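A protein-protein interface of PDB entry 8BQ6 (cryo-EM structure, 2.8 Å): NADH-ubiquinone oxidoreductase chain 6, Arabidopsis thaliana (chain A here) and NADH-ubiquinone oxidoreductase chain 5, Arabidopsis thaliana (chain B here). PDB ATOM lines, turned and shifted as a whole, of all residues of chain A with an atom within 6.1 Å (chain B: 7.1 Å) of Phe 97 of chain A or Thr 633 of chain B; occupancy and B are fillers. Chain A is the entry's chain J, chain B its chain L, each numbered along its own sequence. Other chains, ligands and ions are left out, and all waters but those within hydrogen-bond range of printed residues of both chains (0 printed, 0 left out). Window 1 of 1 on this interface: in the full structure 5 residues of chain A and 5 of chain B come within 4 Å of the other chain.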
ATOM      1  N   ILE A  92     -19.774 -26.254  25.103  1.00  0.00           N
ATOM      2  CA  ILE A  92     -19.433 -26.699  23.753  1.00  0.00           C
ATOM      3  C   ILE A  92     -19.452 -25.529  22.776  1.00  0.00           C
ATOM      4  O   ILE A  92     -18.508 -25.340  21.998  1.00  0.00           O
ATOM      5  CB  ILE A  92     -20.366 -27.834  23.297  1.00  0.00           C
ATOM      6  CG1 ILE A  92     -20.002 -29.142  24.002  1.00  0.00           C
ATOM      7  CG2 ILE A  92     -20.305 -27.996  21.796  1.00  0.00           C
ATOM      8  CD1 ILE A  92     -21.164 -29.823  24.664  1.00  0.00           C
ATOM      9  N   ILE A  93     -20.520 -24.727  22.792  1.00  0.00           N
ATOM     10  CA  ILE A  93     -20.608 -23.623  21.840  1.00  0.00           C
ATOM     11  C   ILE A  93     -19.461 -22.647  22.055  1.00  0.00           C
ATOM     12  O   ILE A  93     -18.747 -22.280  21.110  1.00  0.00           O
ATOM     13  CB  ILE A  93     -21.974 -22.920  21.953  1.00  0.00           C
ATOM     14  CG1 ILE A  93     -23.103 -23.901  21.644  1.00  0.00           C
ATOM     15  CG2 ILE A  93     -22.035 -21.729  21.013  1.00  0.00           C
ATOM     16  CD1 ILE A  93     -23.126 -24.360  20.218  1.00  0.00           C
ATOM     17  N   GLY A  94     -19.252 -22.229  23.305  1.00  0.00           N
ATOM     18  CA  GLY A  94     -18.204 -21.276  23.596  1.00  0.00           C
ATOM     19  C   GLY A  94     -16.825 -21.822  23.302  1.00  0.00           C
ATOM     20  O   GLY A  94     -15.945 -21.089  22.865  1.00  0.00           O
ATOM     21  N   LEU A  95     -16.617 -23.123  23.521  1.00  0.00           N
ATOM     22  CA  LEU A  95     -15.300 -23.695  23.278  1.00  0.00           C
ATOM     23  C   LEU A  95     -15.011 -23.788  21.786  1.00  0.00           C
ATOM     24  O   LEU A  95     -13.896 -23.495  21.343  1.00  0.00           O
ATOM     25  CB  LEU A  95     -15.190 -25.066  23.944  1.00  0.00           C
ATOM     26  CG  LEU A  95     -13.920 -25.860  23.641  1.00  0.00           C
ATOM     27  CD1 LEU A  95     -13.312 -26.370  24.938  1.00  0.00           C
ATOM     28  CD2 LEU A  95     -14.208 -27.008  22.690  1.00  0.00           C
ATOM     29  N   ILE A  96     -16.005 -24.196  20.992  1.00  0.00           N
ATOM     30  CA  ILE A  96     -15.831 -24.188  19.541  1.00  0.00           C
ATOM     31  C   ILE A  96     -15.503 -22.783  19.061  1.00  0.00           C
ATOM     32  O   ILE A  96     -14.525 -22.562  18.333  1.00  0.00           O
ATOM     33  CB  ILE A  96     -17.088 -24.729  18.839  1.00  0.00           C
ATOM     34  CG1 ILE A  96     -17.335 -26.187  19.211  1.00  0.00           C
ATOM     35  CG2 ILE A  96     -16.979 -24.550  17.332  1.00  0.00           C
ATOM     36  CD1 ILE A  96     -18.771 -26.597  19.046  1.00  0.00           C
ATOM     37  N   PHE A  97     -16.307 -21.807  19.486  1.00  0.00           N
ATOM     38  CA  PHE A  97     -16.102 -20.436  19.039  1.00  0.00           C
ATOM     39  C   PHE A  97     -14.771 -19.885  19.539  1.00  0.00           C
ATOM     40  O   PHE A  97     -14.093 -19.143  18.824  1.00  0.00           O
ATOM     41  CB  PHE A  97     -17.270 -19.571  19.504  1.00  0.00           C
ATOM     42  CG  PHE A  97     -18.415 -19.524  18.533  1.00  0.00           C
ATOM     43  CD1 PHE A  97     -19.294 -20.590  18.425  1.00  0.00           C
ATOM     44  CD2 PHE A  97     -18.620 -18.411  17.739  1.00  0.00           C
ATOM     45  CE1 PHE A  97     -20.353 -20.546  17.537  1.00  0.00           C
ATOM     46  CE2 PHE A  97     -19.674 -18.362  16.849  1.00  0.00           C
ATOM     47  CZ  PHE A  97     -20.541 -19.432  16.746  1.00  0.00           C
ATOM     48  N   TRP A  98     -14.362 -20.271  20.749  1.00  0.00           N
ATOM     49  CA  TRP A  98     -13.078 -19.850  21.297  1.00  0.00           C
ATOM     50  C   TRP A  98     -11.927 -20.406  20.474  1.00  0.00           C
ATOM     51  O   TRP A  98     -11.156 -19.648  19.874  1.00  0.00           O
ATOM     52  CB  TRP A  98     -12.975 -20.305  22.756  1.00  0.00           C
ATOM     53  CG  TRP A  98     -11.660 -20.020  23.425  1.00  0.00           C
ATOM     54  CD1 TRP A  98     -11.222 -18.818  23.895  1.00  0.00           C
ATOM     55  CD2 TRP A  98     -10.624 -20.968  23.724  1.00  0.00           C
ATOM     56  NE1 TRP A  98      -9.975 -18.952  24.454  1.00  0.00           N
ATOM     57  CE2 TRP A  98      -9.586 -20.263  24.363  1.00  0.00           C
ATOM     58  CE3 TRP A  98     -10.475 -22.341  23.510  1.00  0.00           C
ATOM     59  CZ2 TRP A  98      -8.412 -20.884  24.786  1.00  0.00           C
ATOM     60  CZ3 TRP A  98      -9.310 -22.953  23.930  1.00  0.00           C
ATOM     61  CH2 TRP A  98      -8.294 -22.226  24.562  1.00  0.00           C
ATOM     62  N   TRP A  99     -11.822 -21.735  20.406  1.00  0.00           N
ATOM     63  CA  TRP A  99     -10.733 -22.374  19.676  1.00  0.00           C
ATOM     64  C   TRP A  99     -10.692 -21.936  18.221  1.00  0.00           C
ATOM     65  O   TRP A  99      -9.613 -21.899  17.619  1.00  0.00           O
ATOM     66  CB  TRP A  99     -10.864 -23.896  19.759  1.00  0.00           C
ATOM     67  CG  TRP A  99      -9.947 -24.629  18.827  1.00  0.00           C
ATOM     68  CD1 TRP A  99     -10.309 -25.473  17.819  1.00  0.00           C
ATOM     69  CD2 TRP A  99      -8.515 -24.582  18.818  1.00  0.00           C
ATOM     70  NE1 TRP A  99      -9.192 -25.955  17.182  1.00  0.00           N
ATOM     71  CE2 TRP A  99      -8.077 -25.423  17.775  1.00  0.00           C
ATOM     72  CE3 TRP A  99      -7.560 -23.908  19.587  1.00  0.00           C
ATOM     73  CZ2 TRP A  99      -6.726 -25.611  17.484  1.00  0.00           C
ATOM     74  CZ3 TRP A  99      -6.218 -24.095  19.296  1.00  0.00           C
ATOM     75  CH2 TRP A  99      -5.816 -24.939  18.254  1.00  0.00           C
ATOM     76  N   GLU A 100     -11.833 -21.583  17.639  1.00  0.00           N
ATOM     77  CA  GLU A 100     -11.788 -21.228  16.231  1.00  0.00           C
ATOM     78  C   GLU A 100     -11.564 -19.740  15.989  1.00  0.00           C
ATOM     79  O   GLU A 100     -10.985 -19.366  14.964  1.00  0.00           O
ATOM     80  CB  GLU A 100     -13.073 -21.679  15.540  1.00  0.00           C
ATOM     81  CG  GLU A 100     -13.041 -21.433  14.068  1.00  0.00           C
ATOM     82  CD  GLU A 100     -12.039 -22.321  13.334  1.00  0.00           C
ATOM     83  OE1 GLU A 100     -12.170 -23.552  13.392  1.00  0.00           O
ATOM     84  OE2 GLU A 100     -11.102 -21.783  12.704  1.00  0.00           O
ATOM     85  N   MET A 101     -12.113 -18.880  16.853  1.00  0.00           N
ATOM     86  CA  MET A 101     -12.088 -17.418  16.539  1.00  0.00           C
ATOM     87  C   MET A 101     -11.121 -16.613  17.402  1.00  0.00           C
ATOM     88  O   MET A 101     -10.687 -15.564  16.922  1.00  0.00           O
ATOM     89  CB  MET A 101     -13.483 -16.807  16.659  1.00  0.00           C
ATOM     90  CG  MET A 101     -14.427 -17.312  15.583  1.00  0.00           C
ATOM     91  SD  MET A 101     -16.102 -16.663  15.766  1.00  0.00           S
ATOM     92  CE  MET A 101     -15.851 -14.959  15.275  1.00  0.00           C
ATOM     93  N   PHE A 102     -10.821 -17.038  18.626  1.00  0.00           N
ATOM     94  CA  PHE A 102      -9.798 -16.311  19.362  1.00  0.00           C
ATOM     95  C   PHE A 102      -8.433 -16.466  18.715  1.00  0.00           C
ATOM     96  O   PHE A 102      -7.500 -15.741  19.075  1.00  0.00           O
ATOM     97  CB  PHE A 102      -9.726 -16.789  20.815  1.00  0.00           C
ATOM     98  CG  PHE A 102     -10.866 -16.322  21.663  1.00  0.00           C
ATOM     99  CD1 PHE A 102     -12.172 -16.560  21.284  1.00  0.00           C
ATOM    100  CD2 PHE A 102     -10.633 -15.633  22.838  1.00  0.00           C
ATOM    101  CE1 PHE A 102     -13.218 -16.138  22.060  1.00  0.00           C
ATOM    102  CE2 PHE A 102     -11.680 -15.202  23.615  1.00  0.00           C
ATOM    103  CZ  PHE A 102     -12.973 -15.455  23.224  1.00  0.00           C
ATOM    104  N   ALA B 627     -31.724 -22.516  16.973  1.00  0.00           N
ATOM    105  CA  ALA B 627     -31.542 -23.162  15.678  1.00  0.00           C
ATOM    106  C   ALA B 627     -30.564 -22.390  14.804  1.00  0.00           C
ATOM    107  O   ALA B 627     -29.714 -22.990  14.135  1.00  0.00           O
ATOM    108  CB  ALA B 627     -32.886 -23.307  14.972  1.00  0.00           C
ATOM    109  N   MET B 628     -30.674 -21.060  14.783  1.00  0.00           N
ATOM    110  CA  MET B 628     -29.714 -20.266  14.018  1.00  0.00           C
ATOM    111  C   MET B 628     -28.296 -20.472  14.534  1.00  0.00           C
ATOM    112  O   MET B 628     -27.353 -20.640  13.750  1.00  0.00           O
ATOM    113  CB  MET B 628     -30.093 -18.787  14.078  1.00  0.00           C
ATOM    114  CG  MET B 628     -31.310 -18.430  13.256  1.00  0.00           C
ATOM    115  SD  MET B 628     -31.877 -16.744  13.547  1.00  0.00           S
ATOM    116  CE  MET B 628     -30.403 -15.808  13.153  1.00  0.00           C
ATOM    117  N   LEU B 629     -28.132 -20.472  15.856  1.00  0.00           N
ATOM    118  CA  LEU B 629     -26.817 -20.658  16.453  1.00  0.00           C
ATOM    119  C   LEU B 629     -26.263 -22.042  16.151  1.00  0.00           C
ATOM    120  O   LEU B 629     -25.065 -22.197  15.891  1.00  0.00           O
ATOM    121  CB  LEU B 629     -26.908 -20.429  17.957  1.00  0.00           C
ATOM    122  CG  LEU B 629     -25.610 -20.458  18.748  1.00  0.00           C
ATOM    123  CD1 LEU B 629     -24.544 -19.645  18.041  1.00  0.00           C
ATOM    124  CD2 LEU B 629     -25.877 -19.909  20.129  1.00  0.00           C
ATOM    125  N   LEU B 630     -27.121 -23.061  16.195  1.00  0.00           N
ATOM    126  CA  LEU B 630     -26.696 -24.417  15.878  1.00  0.00           C
ATOM    127  C   LEU B 630     -26.290 -24.538  14.419  1.00  0.00           C
ATOM    128  O   LEU B 630     -25.324 -25.233  14.097  1.00  0.00           O
ATOM    129  CB  LEU B 630     -27.815 -25.402  16.199  1.00  0.00           C
ATOM    130  CG  LEU B 630     -28.038 -25.709  17.675  1.00  0.00           C
ATOM    131  CD1 LEU B 630     -29.219 -26.644  17.809  1.00  0.00           C
ATOM    132  CD2 LEU B 630     -26.791 -26.312  18.296  1.00  0.00           C
ATOM    133  N   GLY B 631     -27.025 -23.883  13.521  1.00  0.00           N
ATOM    134  CA  GLY B 631     -26.625 -23.876  12.125  1.00  0.00           C
ATOM    135  C   GLY B 631     -25.280 -23.210  11.913  1.00  0.00           C
ATOM    136  O   GLY B 631     -24.438 -23.708  11.162  1.00  0.00           O
ATOM    137  N   LEU B 632     -25.057 -22.075  12.579  1.00  0.00           N
ATOM    138  CA  LEU B 632     -23.752 -21.420  12.515  1.00  0.00           C
ATOM    139  C   LEU B 632     -22.644 -22.335  13.024  1.00  0.00           C
ATOM    140  O   LEU B 632     -21.608 -22.504  12.362  1.00  0.00           O
ATOM    141  CB  LEU B 632     -23.790 -20.127  13.324  1.00  0.00           C
ATOM    142  CG  LEU B 632     -22.603 -19.173  13.245  1.00  0.00           C
ATOM    143  CD1 LEU B 632     -22.359 -18.715  11.822  1.00  0.00           C
ATOM    144  CD2 LEU B 632     -22.877 -17.995  14.149  1.00  0.00           C
ATOM    145  N   THR B 633     -22.850 -22.936  14.200  1.00  0.00           N
ATOM    146  CA  THR B 633     -21.853 -23.828  14.781  1.00  0.00           C
ATOM    147  C   THR B 633     -21.578 -25.010  13.867  1.00  0.00           C
ATOM    148  O   THR B 633     -20.422 -25.398  13.670  1.00  0.00           O
ATOM    149  CB  THR B 633     -22.328 -24.314  16.150  1.00  0.00           C
ATOM    150  OG1 THR B 633     -22.439 -23.197  17.038  1.00  0.00           O
ATOM    151  CG2 THR B 633     -21.351 -25.316  16.732  1.00  0.00           C
ATOM    152  N   LEU B 634     -22.634 -25.590  13.299  1.00  0.00           N
ATOM    153  CA  LEU B 634     -22.492 -26.708  12.378  1.00  0.00           C
ATOM    154  C   LEU B 634     -21.687 -26.318  11.149  1.00  0.00           C
ATOM    155  O   LEU B 634     -20.818 -27.075  10.703  1.00  0.00           O
ATOM    156  CB  LEU B 634     -23.877 -27.203  11.974  1.00  0.00           C
ATOM    157  CG  LEU B 634     -23.984 -28.562  11.298  1.00  0.00           C
ATOM    158  CD1 LEU B 634     -25.152 -29.325  11.881  1.00  0.00           C
ATOM    159  CD2 LEU B 634     -24.154 -28.378   9.805  1.00  0.00           C
ATOM    160  N   PHE B 635     -21.978 -25.148  10.575  1.00  0.00           N
ATOM    161  CA  PHE B 635     -21.219 -24.673   9.423  1.00  0.00           C
ATOM    162  C   PHE B 635     -19.744 -24.560   9.763  1.00  0.00           C
ATOM    163  O   PHE B 635     -18.883 -25.087   9.050  1.00  0.00           O
ATOM    164  CB  PHE B 635     -21.743 -23.310   8.980  1.00  0.00           C
ATOM    165  CG  PHE B 635     -22.889 -23.374   8.024  1.00  0.00           C
ATOM    166  CD1 PHE B 635     -23.666 -24.512   7.919  1.00  0.00           C
ATOM    167  CD2 PHE B 635     -23.220 -22.269   7.263  1.00  0.00           C
ATOM    168  CE1 PHE B 635     -24.734 -24.554   7.049  1.00  0.00           C
ATOM    169  CE2 PHE B 635     -24.286 -22.305   6.395  1.00  0.00           C
ATOM    170  CZ  PHE B 635     -25.045 -23.447   6.288  1.00  0.00           C
ATOM    171  N   VAL B 636     -19.438 -23.866  10.857  1.00  0.00           N
ATOM    172  CA  VAL B 636     -18.046 -23.666  11.249  1.00  0.00           C
ATOM    173  C   VAL B 636     -17.359 -25.007  11.457  1.00  0.00           C
ATOM    174  O   VAL B 636     -16.268 -25.257  10.928  1.00  0.00           O
ATOM    175  CB  VAL B 636     -17.977 -22.785  12.510  1.00  0.00           C
ATOM    176  CG1 VAL B 636     -16.593 -22.829  13.125  1.00  0.00           C
ATOM    177  CG2 VAL B 636     -18.352 -21.366  12.155  1.00  0.00           C
ATOM    178  N   THR B 637     -18.018 -25.910  12.182  1.00  0.00           N
ATOM    179  CA  THR B 637     -17.418 -27.199  12.499  1.00  0.00           C
ATOM    180  C   THR B 637     -17.154 -28.006  11.236  1.00  0.00           C
ATOM    181  O   THR B 637     -16.029 -28.458  11.001  1.00  0.00           O
ATOM    182  CB  THR B 637     -18.329 -27.967  13.455  1.00  0.00           C
ATOM    183  OG1 THR B 637     -18.170 -27.445  14.779  1.00  0.00           O
ATOM    184  CG2 THR B 637     -17.981 -29.445  13.460  1.00  0.00           C
ATOM    185  N   PHE B 638     -18.172 -28.176  10.394  1.00  0.00           N
ATOM    186  CA  PHE B 638     -18.005 -29.062   9.251  1.00  0.00           C
ATOM    187  C   PHE B 638     -17.105 -28.445   8.189  1.00  0.00           C
ATOM    188  O   PHE B 638     -16.216 -29.122   7.662  1.00  0.00           O
ATOM    189  CB  PHE B 638     -19.359 -29.427   8.648  1.00  0.00           C
ATOM    190  CG  PHE B 638     -19.251 -30.246   7.395  1.00  0.00           C
ATOM    191  CD1 PHE B 638     -19.186 -29.643   6.150  1.00  0.00           C
ATOM    192  CD2 PHE B 638     -19.186 -31.624   7.467  1.00  0.00           C
ATOM    193  CE1 PHE B 638     -19.070 -30.399   5.005  1.00  0.00           C
ATOM    194  CE2 PHE B 638     -19.073 -32.381   6.322  1.00  0.00           C
ATOM    195  CZ  PHE B 638     -19.015 -31.769   5.092  1.00  0.00           C
ATOM    196  N   PHE B 639     -17.318 -27.178   7.842  1.00  0.00           N
ATOM    197  CA  PHE B 639     -16.607 -26.619   6.706  1.00  0.00           C
ATOM    198  C   PHE B 639     -15.286 -25.961   7.076  1.00  0.00           C
ATOM    199  O   PHE B 639     -14.539 -25.577   6.171  1.00  0.00           O
ATOM    200  CB  PHE B 639     -17.475 -25.605   5.937  1.00  0.00           C
ATOM    201  CG  PHE B 639     -18.826 -26.134   5.522  1.00  0.00           C
ATOM    202  CD1 PHE B 639     -19.116 -26.317   4.183  1.00  0.00           C
ATOM    203  CD2 PHE B 639     -19.837 -26.337   6.446  1.00  0.00           C
ATOM    204  CE1 PHE B 639     -20.347 -26.793   3.786  1.00  0.00           C
ATOM    205  CE2 PHE B 639     -21.080 -26.792   6.052  1.00  0.00           C
ATOM    206  CZ  PHE B 639     -21.335 -27.017   4.720  1.00  0.00           C
ATOM    207  N   MET B 641     -13.423 -26.806  10.656  1.00  0.00           N
ATOM    208  CA  MET B 641     -12.803 -27.828  11.500  1.00  0.00           C
ATOM    209  C   MET B 641     -13.155 -29.225  11.001  1.00  0.00           C
ATOM    210  O   MET B 641     -13.876 -29.978  11.648  1.00  0.00           O
ATOM    211  CB  MET B 641     -13.231 -27.676  12.954  1.00  0.00           C
ATOM    212  CG  MET B 641     -12.443 -26.697  13.775  1.00  0.00           C
ATOM    213  SD  MET B 641     -13.569 -25.659  14.716  1.00  0.00           S
ATOM    214  CE  MET B 641     -14.294 -26.870  15.805  1.00  0.00           C
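Of the 14 printed residues of chain B, 4 touch a printed residue of chain A.
Among the printed residues, 7 pairs touch across the chains.
Among the printed residues, no Asp or Glu carboxylate lies within 4 Å of a Lys or Arg side-chain nitrogen of the other chain.
Ile 93 of chain A touches Thr 633 of chain B.
CG2 of Thr 633 of chain B touches CD1 of Ile 96 of chain A, at 3.7 Å.
Ile 96 of chain A touches Met 641 of chain B (CG2 to CE, 3.9 Å).
Phe 97 of chain A touches Leu 632 of chain B (CZ to CD2, 3.8 Å).
CE1 of Phe 97 of chain A touches OG1 of Thr 633 of chain B (3.4 Å).
Glu 100 of chain A touches Val 636 of chain B.
Ile 92 of chain A touches none of the printed residues of chain B.
Printed residues of chain B within 4 Å of Ile 93 of chain A: Thr 633 (3.5 Å).
Of the printed residues of chain B, Ile 96 of chain A touches Thr 633 and Met 641.
Of chain B, only Leu 632 and Thr 633 come within 4 Å of Phe 97 of chain A.
Of the printed residues of chain B, Glu 100 of chain A touches Val 636 (3.9 Å) and Met 641 (2.9 Å).
Of the printed residues of chain A, Leu 632 of chain B touches Phe 97 (3.8 Å).
Of the printed residues of chain A, Met 641 of chain B touches Ile 96 and Glu 100.
The nearest residue of chain A that does not touch Thr 633 of chain B is Ile 92 of chain A (5.8 Å).
The side-chain sulfur (SD) of Met 641 of chain B lies close to the side-chain carboxylate (OE1) of Glu 100 of chain A (2.9 Å).
The backbone carbonyl oxygen of Leu 629 of chain B sits at hydrogen-bond distance from the side-chain hydroxyl of Thr 633 of chain B (3.0 Å).
The backbone carbonyl oxygen (O) of Thr 633 of chain B is in hydrogen-bond range of the side-chain hydroxyl (OG1) of Thr 637 of chain B (3.2 Å).
The backbone NH (N) of Met 641 of chain B sits at hydrogen-bond distance from the backbone carbonyl oxygen (O) of Val 636 of chain B.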
